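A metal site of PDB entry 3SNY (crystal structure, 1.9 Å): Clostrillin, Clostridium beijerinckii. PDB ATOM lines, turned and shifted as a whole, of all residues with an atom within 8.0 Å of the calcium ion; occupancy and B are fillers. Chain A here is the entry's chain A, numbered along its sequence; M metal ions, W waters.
N of Asp 80 lies within hydrogen-bond range of O of Met 41.
The side-chain hydroxyl of Thr 42 lies close to the side-chain amide oxygen of Asn 79 (2.6 Å).
The backbone NH (N) of Thr 42 sits at hydrogen-bond distance from the backbone carbonyl oxygen (O) of Tyr 9, 3.0 Å away.
The backbone carbonyl oxygen of Thr 42 sits at hydrogen-bond distance from the backbone NH of Val 74, at 3.0 Å.
The calcium ion is bound by O of Glu 10, water W2, OD1 of Asp 80, OG1 of Thr 42, O of Trp 40, water W1 and water W3.
The calcium ion has seven donor atoms within binding distance.
Four residues have an atom within 4 Å of the calcium ion: Glu 10, Trp 40, Thr 42 and Asp 80.
The nearest printed residue that does not touch the calcium ion is Asn 79 (4.4 Å).
Water W3 bridges OD2 of Asp 80 (2.6 Å) and ND2 of Asn 79 (3.4 Å).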
ATOM      1  N   TYR A   9     -33.684   2.017  16.996  1.00  0.00           N
ATOM      2  CA  TYR A   9     -32.875   0.878  16.561  1.00  0.00           C
ATOM      3  C   TYR A   9     -31.587   0.739  17.355  1.00  0.00           C
ATOM      4  O   TYR A   9     -30.964   1.737  17.742  1.00  0.00           O
ATOM      5  CB  TYR A   9     -32.542   0.990  15.062  1.00  0.00           C
ATOM      6  CG  TYR A   9     -33.737   0.919  14.142  1.00  0.00           C
ATOM      7  CD1 TYR A   9     -34.148  -0.295  13.598  1.00  0.00           C
ATOM      8  CD2 TYR A   9     -34.457   2.061  13.812  1.00  0.00           C
ATOM      9  CE1 TYR A   9     -35.251  -0.359  12.734  1.00  0.00           C
ATOM     10  CE2 TYR A   9     -35.559   2.017  12.960  1.00  0.00           C
ATOM     11  CZ  TYR A   9     -35.944   0.793  12.428  1.00  0.00           C
ATOM     12  OH  TYR A   9     -37.037   0.753  11.577  1.00  0.00           O
ATOM     13  N   GLU A  10     -31.188  -0.503  17.563  1.00  0.00           N
ATOM     14  CA  GLU A  10     -29.971  -0.847  18.301  1.00  0.00           C
ATOM     15  C   GLU A  10     -28.698  -0.398  17.593  1.00  0.00           C
ATOM     16  O   GLU A  10     -27.784   0.129  18.234  1.00  0.00           O
ATOM     17  CB  GLU A  10     -29.923  -2.356  18.540  1.00  0.00           C
ATOM     18  CG  GLU A  10     -28.711  -2.855  19.310  1.00  0.00           C
ATOM     19  CD  GLU A  10     -28.674  -4.367  19.440  1.00  0.00           C
ATOM     20  OE1 GLU A  10     -29.429  -5.063  18.721  1.00  0.00           O
ATOM     21  OE2 GLU A  10     -27.879  -4.872  20.271  1.00  0.00           O
ATOM     22  N   ASP A  11     -28.656  -0.588  16.283  1.00  0.00           N
ATOM     23  CA  ASP A  11     -27.425  -0.379  15.513  1.00  0.00           C
ATOM     24  C   ASP A  11     -27.529   0.750  14.499  1.00  0.00           C
ATOM     25  O   ASP A  11     -28.619   1.253  14.214  1.00  0.00           O
ATOM     26  CB  ASP A  11     -27.008  -1.674  14.800  1.00  0.00           C
ATOM     27  CG  ASP A  11     -26.772  -2.831  15.751  1.00  0.00           C
ATOM     28  OD1 ASP A  11     -26.209  -2.624  16.840  1.00  0.00           O
ATOM     29  OD2 ASP A  11     -27.148  -3.969  15.383  1.00  0.00           O
ATOM     30  N   ILE A  12     -26.372   1.134  13.947  1.00  0.00           N
ATOM     31  CA  ILE A  12     -26.282   2.150  12.897  1.00  0.00           C
ATOM     32  C   ILE A  12     -27.135   1.758  11.694  1.00  0.00           C
ATOM     33  O   ILE A  12     -27.313   0.570  11.405  1.00  0.00           O
ATOM     34  CB  ILE A  12     -24.792   2.400  12.507  1.00  0.00           C
ATOM     35  CG1 ILE A  12     -24.635   3.692  11.685  1.00  0.00           C
ATOM     36  CG2 ILE A  12     -24.184   1.173  11.793  1.00  0.00           C
ATOM     37  CD1 ILE A  12     -23.186   4.158  11.556  1.00  0.00           C
ATOM     38  N   GLY A  15     -30.233  -0.929  11.939  1.00  0.00           N
ATOM     39  CA  GLY A  15     -29.907  -2.356  12.115  1.00  0.00           C
ATOM     40  C   GLY A  15     -30.172  -2.859  13.522  1.00  0.00           C
ATOM     41  O   GLY A  15     -30.423  -2.067  14.437  1.00  0.00           O
ATOM     42  N   ASN A  38     -31.000   0.601  28.520  1.00  0.00           N
ATOM     43  CA  ASN A  38     -30.218   1.818  28.659  1.00  0.00           C
ATOM     44  C   ASN A  38     -29.038   1.827  27.683  1.00  0.00           C
ATOM     45  O   ASN A  38     -28.543   0.765  27.313  1.00  0.00           O
ATOM     46  CB  ASN A  38     -29.682   1.976  30.089  1.00  0.00           C
ATOM     47  CG  ASN A  38     -28.569   0.990  30.415  1.00  0.00           C
ATOM     48  OD1 ASN A  38     -28.808  -0.216  30.544  1.00  0.00           O
ATOM     49  ND2 ASN A  38     -27.351   1.495  30.528  1.00  0.00           N
ATOM     50  N   ASP A  39     -28.613   3.027  27.272  1.00  0.00           N
ATOM     51  CA  ASP A  39     -27.378   3.201  26.514  1.00  0.00           C
ATOM     52  C   ASP A  39     -27.267   2.245  25.317  1.00  0.00           C
ATOM     53  O   ASP A  39     -26.265   1.547  25.152  1.00  0.00           O
ATOM     54  CB  ASP A  39     -26.155   3.057  27.444  1.00  0.00           C
ATOM     55  CG  ASP A  39     -26.171   4.052  28.607  1.00  0.00           C
ATOM     56  OD1 ASP A  39     -26.995   4.985  28.604  1.00  0.00           O
ATOM     57  OD2 ASP A  39     -25.325   3.905  29.516  1.00  0.00           O
ATOM     58  N   TRP A  40     -28.292   2.247  24.478  1.00  0.00           N
ATOM     59  CA  TRP A  40     -28.512   1.202  23.473  1.00  0.00           C
ATOM     60  C   TRP A  40     -28.878   1.774  22.093  1.00  0.00           C
ATOM     61  O   TRP A  40     -28.498   1.219  21.060  1.00  0.00           O
ATOM     62  CB  TRP A  40     -29.602   0.262  23.996  1.00  0.00           C
ATOM     63  CG  TRP A  40     -30.288  -0.688  23.032  1.00  0.00           C
ATOM     64  CD1 TRP A  40     -29.986  -1.997  22.815  1.00  0.00           C
ATOM     65  CD2 TRP A  40     -31.444  -0.408  22.225  1.00  0.00           C
ATOM     66  NE1 TRP A  40     -30.853  -2.546  21.903  1.00  0.00           N
ATOM     67  CE2 TRP A  40     -31.756  -1.590  21.519  1.00  0.00           C
ATOM     68  CE3 TRP A  40     -32.229   0.733  22.008  1.00  0.00           C
ATOM     69  CZ2 TRP A  40     -32.835  -1.673  20.625  1.00  0.00           C
ATOM     70  CZ3 TRP A  40     -33.300   0.655  21.114  1.00  0.00           C
ATOM     71  CH2 TRP A  40     -33.588  -0.534  20.434  1.00  0.00           C
ATOM     72  N   MET A  41     -29.594   2.896  22.091  1.00  0.00           N
ATOM     73  CA  MET A  41     -30.137   3.483  20.862  1.00  0.00           C
ATOM     74  C   MET A  41     -29.078   4.165  19.992  1.00  0.00           C
ATOM     75  O   MET A  41     -28.298   4.987  20.482  1.00  0.00           O
ATOM     76  CB  MET A  41     -31.272   4.458  21.218  1.00  0.00           C
ATOM     77  CG  MET A  41     -32.208   4.785  20.071  1.00  0.00           C
ATOM     78  SD  MET A  41     -31.654   6.187  19.079  1.00  0.00           S
ATOM     79  CE  MET A  41     -31.826   7.539  20.246  1.00  0.00           C
ATOM     80  N   THR A  42     -29.073   3.819  18.711  1.00  0.00           N
ATOM     81  CA  THR A  42     -28.060   4.317  17.756  1.00  0.00           C
ATOM     82  C   THR A  42     -28.666   5.029  16.538  1.00  0.00           C
ATOM     83  O   THR A  42     -28.081   5.952  15.992  1.00  0.00           O
ATOM     84  CB  THR A  42     -27.105   3.177  17.321  1.00  0.00           C
ATOM     85  OG1 THR A  42     -26.366   2.729  18.461  1.00  0.00           O
ATOM     86  CG2 THR A  42     -26.110   3.638  16.261  1.00  0.00           C
ATOM     87  N   SER A  43     -29.842   4.562  16.110  1.00  0.00           N
ATOM     88  CA  SER A  43     -30.567   5.198  15.007  1.00  0.00           C
ATOM     89  C   SER A  43     -32.067   5.149  15.263  1.00  0.00           C
ATOM     90  O   SER A  43     -32.536   4.370  16.097  1.00  0.00           O
ATOM     91  CB  SER A  43     -30.226   4.525  13.672  1.00  0.00           C
ATOM     92  OG  SER A  43     -30.607   3.159  13.656  1.00  0.00           O
ATOM     93  N   TRP A  73     -27.857   7.694  12.113  1.00  0.00           N
ATOM     94  CA  TRP A  73     -26.806   7.768  13.119  1.00  0.00           C
ATOM     95  C   TRP A  73     -27.069   8.994  13.992  1.00  0.00           C
ATOM     96  O   TRP A  73     -27.106  10.122  13.500  1.00  0.00           O
ATOM     97  CB  TRP A  73     -25.432   7.852  12.450  1.00  0.00           C
ATOM     98  CG  TRP A  73     -24.290   8.185  13.373  1.00  0.00           C
ATOM     99  CD1 TRP A  73     -23.642   9.385  13.472  1.00  0.00           C
ATOM    100  CD2 TRP A  73     -23.658   7.313  14.319  1.00  0.00           C
ATOM    101  NE1 TRP A  73     -22.645   9.310  14.416  1.00  0.00           N
ATOM    102  CE2 TRP A  73     -22.639   8.057  14.956  1.00  0.00           C
ATOM    103  CE3 TRP A  73     -23.863   5.973  14.693  1.00  0.00           C
ATOM    104  CZ2 TRP A  73     -21.824   7.505  15.947  1.00  0.00           C
ATOM    105  CZ3 TRP A  73     -23.048   5.421  15.684  1.00  0.00           C
ATOM    106  CH2 TRP A  73     -22.041   6.194  16.294  1.00  0.00           C
ATOM    107  N   VAL A  74     -27.246   8.760  15.299  1.00  0.00           N
ATOM    108  CA  VAL A  74     -27.635   9.825  16.232  1.00  0.00           C
ATOM    109  C   VAL A  74     -26.519  10.836  16.533  1.00  0.00           C
ATOM    110  O   VAL A  74     -26.777  11.907  17.095  1.00  0.00           O
ATOM    111  CB  VAL A  74     -28.213   9.266  17.555  1.00  0.00           C
ATOM    112  CG1 VAL A  74     -29.577   8.650  17.318  1.00  0.00           C
ATOM    113  CG2 VAL A  74     -27.259   8.273  18.197  1.00  0.00           C
ATOM    114  N   ASN A  79     -24.744   8.670  20.737  1.00  0.00           N
ATOM    115  CA  ASN A  79     -24.752   7.212  20.558  1.00  0.00           C
ATOM    116  C   ASN A  79     -24.698   6.427  21.860  1.00  0.00           C
ATOM    117  O   ASN A  79     -23.833   6.676  22.708  1.00  0.00           O
ATOM    118  CB  ASN A  79     -23.639   6.743  19.624  1.00  0.00           C
ATOM    119  CG  ASN A  79     -23.752   5.276  19.293  1.00  0.00           C
ATOM    120  OD1 ASN A  79     -24.848   4.780  19.010  1.00  0.00           O
ATOM    121  ND2 ASN A  79     -22.642   4.550  19.327  1.00  0.00           N
ATOM    122  N   ASP A  80     -25.609   5.465  21.994  1.00  0.00           N
ATOM    123  CA  ASP A  80     -25.703   4.611  23.189  1.00  0.00           C
ATOM    124  C   ASP A  80     -25.762   5.420  24.484  1.00  0.00           C
ATOM    125  O   ASP A  80     -25.013   5.146  25.431  1.00  0.00           O
ATOM    126  CB  ASP A  80     -24.541   3.600  23.231  1.00  0.00           C
ATOM    127  CG  ASP A  80     -24.628   2.552  22.131  1.00  0.00           C
ATOM    128  OD1 ASP A  80     -25.678   2.436  21.476  1.00  0.00           O
ATOM    129  OD2 ASP A  80     -23.621   1.827  21.934  1.00  0.00           O
ATOM    130  N   LYS A  81     -26.642   6.415  24.523  1.00  0.00           N
ATOM    131  CA  LYS A  81     -26.771   7.272  25.708  1.00  0.00           C
ATOM    132  C   LYS A  81     -28.209   7.436  26.213  1.00  0.00           C
ATOM    133  O   LYS A  81     -28.402   7.893  27.345  1.00  0.00           O
ATOM    134  CB  LYS A  81     -26.153   8.661  25.462  1.00  0.00           C
ATOM    135  CG  LYS A  81     -24.621   8.693  25.321  1.00  0.00           C
ATOM    136  CD  LYS A  81     -23.897   8.189  26.573  1.00  0.00           C
ATOM    137  CE  LYS A  81     -23.934   9.186  27.718  1.00  0.00           C
ATOM    138  NZ  LYS A  81     -23.613   8.556  29.034  1.00  0.00           N
HETATM  139 CA    CA M   1     -26.249   0.738  19.880  1.00  0.00          CA
HETATM  140  O   HOH W   1     -24.822  -0.713  18.136  1.00  0.00           O
HETATM  141  O   HOH W   2     -25.869  -1.143  21.260  1.00  0.00           O
HETATM  142  O   HOH W   3     -23.611   1.336  19.381  1.00  0.00           O
